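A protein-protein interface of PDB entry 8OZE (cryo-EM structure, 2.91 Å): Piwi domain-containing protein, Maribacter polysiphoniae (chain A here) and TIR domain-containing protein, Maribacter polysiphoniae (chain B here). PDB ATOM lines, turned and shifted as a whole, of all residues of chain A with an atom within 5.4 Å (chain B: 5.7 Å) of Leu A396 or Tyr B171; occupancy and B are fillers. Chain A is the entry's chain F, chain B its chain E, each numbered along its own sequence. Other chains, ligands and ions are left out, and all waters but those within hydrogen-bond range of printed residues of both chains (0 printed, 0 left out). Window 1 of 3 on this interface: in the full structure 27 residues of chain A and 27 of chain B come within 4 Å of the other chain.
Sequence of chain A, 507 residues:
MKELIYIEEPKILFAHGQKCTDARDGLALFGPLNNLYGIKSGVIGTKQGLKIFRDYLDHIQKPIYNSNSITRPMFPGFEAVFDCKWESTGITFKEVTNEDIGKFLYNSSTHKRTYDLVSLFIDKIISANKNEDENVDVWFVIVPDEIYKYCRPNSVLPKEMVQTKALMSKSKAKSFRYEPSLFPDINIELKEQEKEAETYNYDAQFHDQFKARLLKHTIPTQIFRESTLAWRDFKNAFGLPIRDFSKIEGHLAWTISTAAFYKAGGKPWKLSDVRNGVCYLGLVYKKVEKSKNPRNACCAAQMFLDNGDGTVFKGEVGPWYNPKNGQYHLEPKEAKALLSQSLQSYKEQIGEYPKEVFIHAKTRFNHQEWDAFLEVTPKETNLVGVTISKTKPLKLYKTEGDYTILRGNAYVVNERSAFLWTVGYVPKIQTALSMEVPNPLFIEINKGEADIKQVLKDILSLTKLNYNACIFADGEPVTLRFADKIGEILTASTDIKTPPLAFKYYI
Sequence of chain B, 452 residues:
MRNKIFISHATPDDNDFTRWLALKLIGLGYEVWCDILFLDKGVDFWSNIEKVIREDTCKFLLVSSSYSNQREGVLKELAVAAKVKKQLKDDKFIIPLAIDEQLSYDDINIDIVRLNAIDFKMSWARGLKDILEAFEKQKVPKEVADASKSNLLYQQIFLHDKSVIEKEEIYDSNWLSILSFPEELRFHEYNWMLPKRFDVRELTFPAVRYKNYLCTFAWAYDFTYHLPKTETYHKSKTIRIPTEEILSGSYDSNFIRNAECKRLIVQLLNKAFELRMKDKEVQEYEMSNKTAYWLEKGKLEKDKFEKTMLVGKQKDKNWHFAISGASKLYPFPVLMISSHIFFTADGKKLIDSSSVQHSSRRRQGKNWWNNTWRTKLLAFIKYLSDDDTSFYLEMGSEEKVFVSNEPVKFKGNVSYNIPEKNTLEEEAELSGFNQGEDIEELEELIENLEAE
Of the 12 printed residues of chain A, 10 touch a printed residue of chain B. Hydrophobic or aromatic side chains of chain A that line the printed part of chain B: Leu A4, Leu A396, Tyr A397, Ile A405 and Leu A406. Printed residues of chain B that touch a printed residue of chain A: Glu B169, Ile B170, Tyr B171, Asp B172, Ser B173, Asn B174, Asn B370, Phe B410, Lys B411, Gly B412 and Val B414. Hydrophobic or aromatic side chains of chain B that line the printed part of chain A: Tyr B171, Phe B410 and Val B414. Among the printed residues, no Asp or Glu carboxylate lies within 4 Å of a Lys or Arg side-chain nitrogen of the other chain.
OG of Ser B173 lies within hydrogen-bond range of O of Val B408 (2.8 Å). The backbone carbonyl oxygen (O) of Phe B410 lies within hydrogen-bond range of the backbone NH (N) of Tyr B171, 2.6 Å away. The backbone carbonyl oxygen of Gly B412 is in hydrogen-bond range of the backbone NH of Glu B169 (2.6 Å). N of Trp A421 sits at hydrogen-bond distance from O of Asn A409 (3.0 Å). The backbone carbonyl oxygen (O) of Leu A406 lies close to the side-chain amide oxygen (OD1) of Asn A409, at 3.4 Å. The side-chain hydroxyl (OH) of Tyr B171 sits at hydrogen-bond distance from the backbone carbonyl oxygen (O) of Val B414 (3.5 Å).
Of the printed residues of chain B, Lys A398 touches Glu B169, Tyr B171 and Asn B370. Of the printed residues of chain B, Thr A399 touches Glu B169 (3.1 Å), Ile B170 (3.2 Å) and Asp B172 (3.9 Å). Trp A421 touches none of the printed residues of chain B. Of chain A, only Leu A4, Leu A396, Tyr A397, Lys A398, Ile A405 and Asn A409 come within 4 Å of Tyr B171. Val B408 touches none of the printed residues of chain A. The nearest residue of chain B that does not touch Leu A396 is Asn B174 (4.8 Å). The nearest printed residue of chain A that does not touch Ser B173 is Leu A394 (4.1 Å).
The side-chain carboxylate of Glu B169 sits at hydrogen-bond distance from the side-chain hydroxyl of Thr A399 (3.1 Å). N of Lys A398 lies close to ND2 of Asn B370, 3.2 Å away. N of Tyr A397 sits at hydrogen-bond distance from O of Asp B172 (2.6 Å). The backbone carbonyl oxygen (O) of Lys B411 lies within hydrogen-bond range of the backbone NH (N) of Leu A4 (3.2 Å). OD1 of Asn B174 is in hydrogen-bond range of N of Lys A395.
Gly B412 touches Leu A4. Lys A395 touches Ser B173. CB of Tyr B171 touches CB of Leu A396, at 3.97 Å. Leu A396 touches Ser B173. Asn B370 touches Tyr A397. O of Ile B170 touches CG2 of Thr A399 (3.2 Å). CG2 of Thr A399 touches OD1 of Asp B172, 3.9 Å away. Tyr B171 touches Ile A405 (CE1 to CG1, 3.5 Å). Val B414 touches Leu A406. ND2 of Asn A409 touches CG2 of Val B414, 3.9 Å away.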
ATOM      1  N   LEU A   4      -8.363  -3.612 -16.119  1.00  0.00           N
ATOM      2  CA  LEU A   4      -7.656  -3.371 -14.866  1.00  0.00           C
ATOM      3  C   LEU A   4      -8.586  -2.595 -13.944  1.00  0.00           C
ATOM      4  O   LEU A   4      -8.715  -1.374 -14.077  1.00  0.00           O
ATOM      5  CB  LEU A   4      -6.360  -2.603 -15.129  1.00  0.00           C
ATOM      6  CG  LEU A   4      -5.394  -2.307 -13.988  1.00  0.00           C
ATOM      7  CD1 LEU A   4      -4.859  -3.600 -13.423  1.00  0.00           C
ATOM      8  CD2 LEU A   4      -4.256  -1.438 -14.481  1.00  0.00           C
ATOM      9  N   LEU A 394       5.497  -9.252 -12.155  1.00  0.00           N
ATOM     10  CA  LEU A 394       4.683  -8.339 -12.948  1.00  0.00           C
ATOM     11  C   LEU A 394       5.009  -6.909 -12.546  1.00  0.00           C
ATOM     12  O   LEU A 394       5.113  -6.605 -11.354  1.00  0.00           O
ATOM     13  CB  LEU A 394       3.191  -8.618 -12.764  1.00  0.00           C
ATOM     14  CG  LEU A 394       2.217  -7.658 -13.452  1.00  0.00           C
ATOM     15  CD1 LEU A 394       2.534  -7.525 -14.926  1.00  0.00           C
ATOM     16  CD2 LEU A 394       0.783  -8.115 -13.267  1.00  0.00           C
ATOM     17  N   LYS A 395       5.195  -6.042 -13.536  1.00  0.00           N
ATOM     18  CA  LYS A 395       5.433  -4.622 -13.293  1.00  0.00           C
ATOM     19  C   LYS A 395       4.756  -3.834 -14.403  1.00  0.00           C
ATOM     20  O   LYS A 395       5.083  -4.014 -15.578  1.00  0.00           O
ATOM     21  CB  LYS A 395       6.926  -4.300 -13.238  1.00  0.00           C
ATOM     22  CG  LYS A 395       7.602  -4.659 -11.933  1.00  0.00           C
ATOM     23  CD  LYS A 395       9.048  -4.210 -11.936  1.00  0.00           C
ATOM     24  CE  LYS A 395       9.705  -4.474 -10.598  1.00  0.00           C
ATOM     25  NZ  LYS A 395       9.771  -5.929 -10.300  1.00  0.00           N
ATOM     26  N   LEU A 396       3.821  -2.965 -14.036  1.00  0.00           N
ATOM     27  CA  LEU A 396       3.170  -2.083 -14.999  1.00  0.00           C
ATOM     28  C   LEU A 396       3.894  -0.746 -14.990  1.00  0.00           C
ATOM     29  O   LEU A 396       3.860  -0.013 -13.999  1.00  0.00           O
ATOM     30  CB  LEU A 396       1.691  -1.909 -14.683  1.00  0.00           C
ATOM     31  CG  LEU A 396       0.819  -3.142 -14.878  1.00  0.00           C
ATOM     32  CD1 LEU A 396      -0.616  -2.833 -14.508  1.00  0.00           C
ATOM     33  CD2 LEU A 396       0.917  -3.599 -16.305  1.00  0.00           C
ATOM     34  N   TYR A 397       4.553  -0.430 -16.095  1.00  0.00           N
ATOM     35  CA  TYR A 397       5.137   0.886 -16.297  1.00  0.00           C
ATOM     36  C   TYR A 397       4.163   1.720 -17.117  1.00  0.00           C
ATOM     37  O   TYR A 397       3.746   1.303 -18.202  1.00  0.00           O
ATOM     38  CB  TYR A 397       6.486   0.781 -17.002  1.00  0.00           C
ATOM     39  CG  TYR A 397       7.382  -0.318 -16.482  1.00  0.00           C
ATOM     40  CD1 TYR A 397       8.249  -0.088 -15.426  1.00  0.00           C
ATOM     41  CD2 TYR A 397       7.371  -1.580 -17.055  1.00  0.00           C
ATOM     42  CE1 TYR A 397       9.074  -1.086 -14.951  1.00  0.00           C
ATOM     43  CE2 TYR A 397       8.192  -2.584 -16.586  1.00  0.00           C
ATOM     44  CZ  TYR A 397       9.041  -2.331 -15.534  1.00  0.00           C
ATOM     45  OH  TYR A 397       9.862  -3.324 -15.059  1.00  0.00           O
ATOM     46  N   LYS A 398       3.796   2.888 -16.598  1.00  0.00           N
ATOM     47  CA  LYS A 398       2.867   3.747 -17.310  1.00  0.00           C
ATOM     48  C   LYS A 398       3.529   4.318 -18.562  1.00  0.00           C
ATOM     49  O   LYS A 398       4.756   4.417 -18.658  1.00  0.00           O
ATOM     50  CB  LYS A 398       2.374   4.872 -16.402  1.00  0.00           C
ATOM     51  CG  LYS A 398       1.037   5.450 -16.820  1.00  0.00           C
ATOM     52  CD  LYS A 398       0.583   6.547 -15.880  1.00  0.00           C
ATOM     53  CE  LYS A 398       0.173   5.981 -14.536  1.00  0.00           C
ATOM     54  NZ  LYS A 398      -0.418   7.028 -13.664  1.00  0.00           N
ATOM     55  N   THR A 399       2.694   4.691 -19.534  1.00  0.00           N
ATOM     56  CA  THR A 399       3.201   5.095 -20.843  1.00  0.00           C
ATOM     57  C   THR A 399       4.115   6.311 -20.740  1.00  0.00           C
ATOM     58  O   THR A 399       5.228   6.310 -21.275  1.00  0.00           O
ATOM     59  CB  THR A 399       2.038   5.383 -21.791  1.00  0.00           C
ATOM     60  OG1 THR A 399       1.077   6.218 -21.132  1.00  0.00           O
ATOM     61  CG2 THR A 399       1.369   4.089 -22.223  1.00  0.00           C
ATOM     62  N   ILE A 405       2.297   3.262 -11.045  1.00  0.00           N
ATOM     63  CA  ILE A 405       0.860   3.057 -11.150  1.00  0.00           C
ATOM     64  C   ILE A 405       0.160   3.514  -9.872  1.00  0.00           C
ATOM     65  O   ILE A 405       0.758   3.626  -8.796  1.00  0.00           O
ATOM     66  CB  ILE A 405       0.562   1.578 -11.454  1.00  0.00           C
ATOM     67  CG1 ILE A 405      -0.887   1.383 -11.904  1.00  0.00           C
ATOM     68  CG2 ILE A 405       0.868   0.724 -10.247  1.00  0.00           C
ATOM     69  CD1 ILE A 405      -1.251  -0.053 -12.181  1.00  0.00           C
ATOM     70  N   LEU A 406      -1.130   3.801 -10.007  1.00  0.00           N
ATOM     71  CA  LEU A 406      -1.974   4.109  -8.864  1.00  0.00           C
ATOM     72  C   LEU A 406      -2.107   2.893  -7.954  1.00  0.00           C
ATOM     73  O   LEU A 406      -2.186   1.752  -8.414  1.00  0.00           O
ATOM     74  CB  LEU A 406      -3.356   4.555  -9.345  1.00  0.00           C
ATOM     75  CG  LEU A 406      -4.385   5.051  -8.331  1.00  0.00           C
ATOM     76  CD1 LEU A 406      -4.013   6.426  -7.809  1.00  0.00           C
ATOM     77  CD2 LEU A 406      -5.771   5.065  -8.951  1.00  0.00           C
ATOM     78  N   ASN A 409      -5.186  -0.425  -7.982  1.00  0.00           N
ATOM     79  CA  ASN A 409      -5.474  -1.076  -9.249  1.00  0.00           C
ATOM     80  C   ASN A 409      -5.322  -2.583  -9.111  1.00  0.00           C
ATOM     81  O   ASN A 409      -4.377  -3.074  -8.489  1.00  0.00           O
ATOM     82  CB  ASN A 409      -4.544  -0.555 -10.342  1.00  0.00           C
ATOM     83  CG  ASN A 409      -5.059   0.710 -10.984  1.00  0.00           C
ATOM     84  OD1 ASN A 409      -4.377   1.732 -10.999  1.00  0.00           O
ATOM     85  ND2 ASN A 409      -6.273   0.652 -11.518  1.00  0.00           N
ATOM     86  N   TRP A 421      -2.416  -3.909  -6.438  1.00  0.00           N
ATOM     87  CA  TRP A 421      -1.321  -2.979  -6.170  1.00  0.00           C
ATOM     88  C   TRP A 421      -1.580  -2.295  -4.835  1.00  0.00           C
ATOM     89  O   TRP A 421      -2.165  -1.216  -4.767  1.00  0.00           O
ATOM     90  CB  TRP A 421      -1.180  -1.971  -7.301  1.00  0.00           C
ATOM     91  CG  TRP A 421      -0.224  -2.407  -8.357  1.00  0.00           C
ATOM     92  CD1 TRP A 421       1.094  -2.084  -8.449  1.00  0.00           C
ATOM     93  CD2 TRP A 421      -0.507  -3.263  -9.468  1.00  0.00           C
ATOM     94  NE1 TRP A 421       1.652  -2.677  -9.553  1.00  0.00           N
ATOM     95  CE2 TRP A 421       0.688  -3.409 -10.196  1.00  0.00           C
ATOM     96  CE3 TRP A 421      -1.654  -3.918  -9.921  1.00  0.00           C
ATOM     97  CZ2 TRP A 421       0.768  -4.181 -11.347  1.00  0.00           C
ATOM     98  CZ3 TRP A 421      -1.572  -4.683 -11.063  1.00  0.00           C
ATOM     99  CH2 TRP A 421      -0.369  -4.812 -11.762  1.00  0.00           C
ATOM    100  N   VAL A 437       9.696   0.846  -9.324  1.00  0.00           N
ATOM    101  CA  VAL A 437       8.405   0.332  -9.772  1.00  0.00           C
ATOM    102  C   VAL A 437       7.998  -0.812  -8.851  1.00  0.00           C
ATOM    103  O   VAL A 437       8.721  -1.813  -8.748  1.00  0.00           O
ATOM    104  CB  VAL A 437       8.461  -0.114 -11.239  1.00  0.00           C
ATOM    105  CG1 VAL A 437       7.080  -0.529 -11.716  1.00  0.00           C
ATOM    106  CG2 VAL A 437       9.013   1.008 -12.101  1.00  0.00           C
ATOM    107  N   GLU B 169      -6.345   4.855 -18.874  1.00  0.00           N
ATOM    108  CA  GLU B 169      -4.892   4.906 -18.939  1.00  0.00           C
ATOM    109  C   GLU B 169      -4.355   3.555 -19.386  1.00  0.00           C
ATOM    110  O   GLU B 169      -4.849   2.510 -18.958  1.00  0.00           O
ATOM    111  CB  GLU B 169      -4.288   5.295 -17.583  1.00  0.00           C
ATOM    112  CG  GLU B 169      -2.773   5.407 -17.585  1.00  0.00           C
ATOM    113  CD  GLU B 169      -2.276   6.550 -18.445  1.00  0.00           C
ATOM    114  OE1 GLU B 169      -3.008   7.550 -18.590  1.00  0.00           O
ATOM    115  OE2 GLU B 169      -1.152   6.447 -18.979  1.00  0.00           O
ATOM    116  N   ILE B 170      -3.343   3.586 -20.249  1.00  0.00           N
ATOM    117  CA  ILE B 170      -2.715   2.384 -20.784  1.00  0.00           C
ATOM    118  C   ILE B 170      -1.390   2.166 -20.070  1.00  0.00           C
ATOM    119  O   ILE B 170      -0.609   3.107 -19.887  1.00  0.00           O
ATOM    120  CB  ILE B 170      -2.512   2.492 -22.306  1.00  0.00           C
ATOM    121  CG1 ILE B 170      -3.827   2.861 -22.993  1.00  0.00           C
ATOM    122  CG2 ILE B 170      -1.972   1.188 -22.866  1.00  0.00           C
ATOM    123  CD1 ILE B 170      -4.913   1.826 -22.830  1.00  0.00           C
ATOM    124  N   TYR B 171      -1.138   0.926 -19.661  1.00  0.00           N
ATOM    125  CA  TYR B 171       0.060   0.572 -18.919  1.00  0.00           C
ATOM    126  C   TYR B 171       0.883  -0.440 -19.703  1.00  0.00           C
ATOM    127  O   TYR B 171       0.338  -1.339 -20.349  1.00  0.00           O
ATOM    128  CB  TYR B 171      -0.291  -0.007 -17.546  1.00  0.00           C
ATOM    129  CG  TYR B 171      -1.072   0.936 -16.665  1.00  0.00           C
ATOM    130  CD1 TYR B 171      -0.428   1.882 -15.882  1.00  0.00           C
ATOM    131  CD2 TYR B 171      -2.457   0.881 -16.616  1.00  0.00           C
ATOM    132  CE1 TYR B 171      -1.141   2.745 -15.078  1.00  0.00           C
ATOM    133  CE2 TYR B 171      -3.177   1.738 -15.815  1.00  0.00           C
ATOM    134  CZ  TYR B 171      -2.515   2.668 -15.048  1.00  0.00           C
ATOM    135  OH  TYR B 171      -3.232   3.524 -14.247  1.00  0.00           O
ATOM    136  N   ASP B 172       2.202  -0.291 -19.635  1.00  0.00           N
ATOM    137  CA  ASP B 172       3.135  -1.191 -20.298  1.00  0.00           C
ATOM    138  C   ASP B 172       3.693  -2.165 -19.271  1.00  0.00           C
ATOM    139  O   ASP B 172       4.385  -1.754 -18.333  1.00  0.00           O
ATOM    140  CB  ASP B 172       4.269  -0.414 -20.965  1.00  0.00           C
ATOM    141  CG  ASP B 172       3.850   0.220 -22.271  1.00  0.00           C
ATOM    142  OD1 ASP B 172       2.635   0.417 -22.475  1.00  0.00           O
ATOM    143  OD2 ASP B 172       4.737   0.515 -23.099  1.00  0.00           O
ATOM    144  N   SER B 173       3.401  -3.448 -19.453  1.00  0.00           N
ATOM    145  CA  SER B 173       3.892  -4.475 -18.552  1.00  0.00           C
ATOM    146  C   SER B 173       5.272  -4.941 -19.000  1.00  0.00           C
ATOM    147  O   SER B 173       5.815  -4.483 -20.006  1.00  0.00           O
ATOM    148  CB  SER B 173       2.915  -5.645 -18.494  1.00  0.00           C
ATOM    149  OG  SER B 173       3.137  -6.535 -19.571  1.00  0.00           O
ATOM    150  N   ASN B 174       5.854  -5.864 -18.237  1.00  0.00           N
ATOM    151  CA  ASN B 174       7.117  -6.494 -18.595  1.00  0.00           C
ATOM    152  C   ASN B 174       6.916  -7.888 -19.177  1.00  0.00           C
ATOM    153  O   ASN B 174       7.882  -8.646 -19.308  1.00  0.00           O
ATOM    154  CB  ASN B 174       8.044  -6.551 -17.382  1.00  0.00           C
ATOM    155  CG  ASN B 174       7.388  -7.184 -16.176  1.00  0.00           C
ATOM    156  OD1 ASN B 174       6.384  -6.688 -15.669  1.00  0.00           O
ATOM    157  ND2 ASN B 174       7.955  -8.289 -15.708  1.00  0.00           N
ATOM    158  N   ASN B 370      10.072   6.006 -13.467  1.00  0.00           N
ATOM    159  CA  ASN B 370       9.257   5.141 -14.320  1.00  0.00           C
ATOM    160  C   ASN B 370       9.778   5.087 -15.752  1.00  0.00           C
ATOM    161  O   ASN B 370      10.015   4.002 -16.298  1.00  0.00           O
ATOM    162  CB  ASN B 370       7.809   5.632 -14.303  1.00  0.00           C
ATOM    163  CG  ASN B 370       6.854   4.664 -14.963  1.00  0.00           C
ATOM    164  OD1 ASN B 370       7.244   3.580 -15.392  1.00  0.00           O
ATOM    165  ND2 ASN B 370       5.589   5.056 -15.058  1.00  0.00           N
ATOM    166  N   VAL B 408       2.782  -6.946 -23.202  1.00  0.00           N
ATOM    167  CA  VAL B 408       1.351  -6.929 -22.933  1.00  0.00           C
ATOM    168  C   VAL B 408       0.974  -5.587 -22.331  1.00  0.00           C
ATOM    169  O   VAL B 408       1.639  -5.087 -21.416  1.00  0.00           O
ATOM    170  CB  VAL B 408       0.969  -8.085 -21.998  1.00  0.00           C
ATOM    171  CG1 VAL B 408      -0.532  -8.113 -21.777  1.00  0.00           C
ATOM    172  CG2 VAL B 408       1.450  -9.403 -22.562  1.00  0.00           C
ATOM    173  N   LYS B 409      -0.092  -4.992 -22.847  1.00  0.00           N
ATOM    174  CA  LYS B 409      -0.566  -3.703 -22.370  1.00  0.00           C
ATOM    175  C   LYS B 409      -1.833  -3.890 -21.550  1.00  0.00           C
ATOM    176  O   LYS B 409      -2.673  -4.735 -21.869  1.00  0.00           O
ATOM    177  CB  LYS B 409      -0.829  -2.751 -23.536  1.00  0.00           C
ATOM    178  CG  LYS B 409       0.426  -2.315 -24.266  1.00  0.00           C
ATOM    179  CD  LYS B 409       0.126  -1.224 -25.275  1.00  0.00           C
ATOM    180  CE  LYS B 409       1.385  -0.790 -26.003  1.00  0.00           C
ATOM    181  NZ  LYS B 409       2.349  -0.130 -25.083  1.00  0.00           N
ATOM    182  N   PHE B 410      -1.962  -3.102 -20.490  1.00  0.00           N
ATOM    183  CA  PHE B 410      -3.120  -3.138 -19.613  1.00  0.00           C
ATOM    184  C   PHE B 410      -3.787  -1.770 -19.604  1.00  0.00           C
ATOM    185  O   PHE B 410      -3.127  -0.729 -19.664  1.00  0.00           O
ATOM    186  CB  PHE B 410      -2.722  -3.556 -18.191  1.00  0.00           C
ATOM    187  CG  PHE B 410      -2.247  -4.978 -18.086  1.00  0.00           C
ATOM    188  CD1 PHE B 410      -0.978  -5.332 -18.504  1.00  0.00           C
ATOM    189  CD2 PHE B 410      -3.065  -5.957 -17.562  1.00  0.00           C
ATOM    190  CE1 PHE B 410      -0.537  -6.633 -18.403  1.00  0.00           C
ATOM    191  CE2 PHE B 410      -2.628  -7.261 -17.461  1.00  0.00           C
ATOM    192  CZ  PHE B 410      -1.363  -7.598 -17.883  1.00  0.00           C
ATOM    193  N   LYS B 411      -5.116  -1.777 -19.528  1.00  0.00           N
ATOM    194  CA  LYS B 411      -5.908  -0.554 -19.635  1.00  0.00           C
ATOM    195  C   LYS B 411      -6.606  -0.304 -18.306  1.00  0.00           C
ATOM    196  O   LYS B 411      -7.456  -1.097 -17.891  1.00  0.00           O
ATOM    197  CB  LYS B 411      -6.924  -0.652 -20.771  1.00  0.00           C
ATOM    198  CG  LYS B 411      -7.798   0.579 -20.927  1.00  0.00           C
ATOM    199  CD  LYS B 411      -8.917   0.342 -21.925  1.00  0.00           C
ATOM    200  CE  LYS B 411      -8.392   0.341 -23.352  1.00  0.00           C
ATOM    201  NZ  LYS B 411      -9.494   0.245 -24.347  1.00  0.00           N
ATOM    202  N   GLY B 412      -6.257   0.796 -17.649  1.00  0.00           N
ATOM    203  CA  GLY B 412      -6.869   1.175 -16.386  1.00  0.00           C
ATOM    204  C   GLY B 412      -7.864   2.305 -16.584  1.00  0.00           C
ATOM    205  O   GLY B 412      -7.618   3.238 -17.347  1.00  0.00           O
ATOM    206  N   VAL B 414      -8.878   4.452 -14.313  1.00  0.00           N
ATOM    207  CA  VAL B 414      -8.628   5.589 -13.437  1.00  0.00           C
ATOM    208  C   VAL B 414      -7.165   5.986 -13.566  1.00  0.00           C
ATOM    209  O   VAL B 414      -6.284   5.126 -13.674  1.00  0.00           O
ATOM    210  CB  VAL B 414      -8.981   5.272 -11.970  1.00  0.00           C
ATOM    211  CG1 VAL B 414     -10.488   5.201 -11.791  1.00  0.00           C
ATOM    212  CG2 VAL B 414      -8.333   3.973 -11.539  1.00  0.00           C
ATOM    213  N   SER B 415      -6.908   7.291 -13.565  1.00  0.00           N
ATOM    214  CA  SER B 415      -5.555   7.817 -13.691  1.00  0.00           C
ATOM    215  C   SER B 415      -5.428   9.030 -12.776  1.00  0.00           C
ATOM    216  O   SER B 415      -6.273   9.270 -11.908  1.00  0.00           O
ATOM    217  CB  SER B 415      -5.237   8.151 -15.154  1.00  0.00           C
ATOM    218  OG  SER B 415      -5.674   9.457 -15.487  1.00  0.00           O
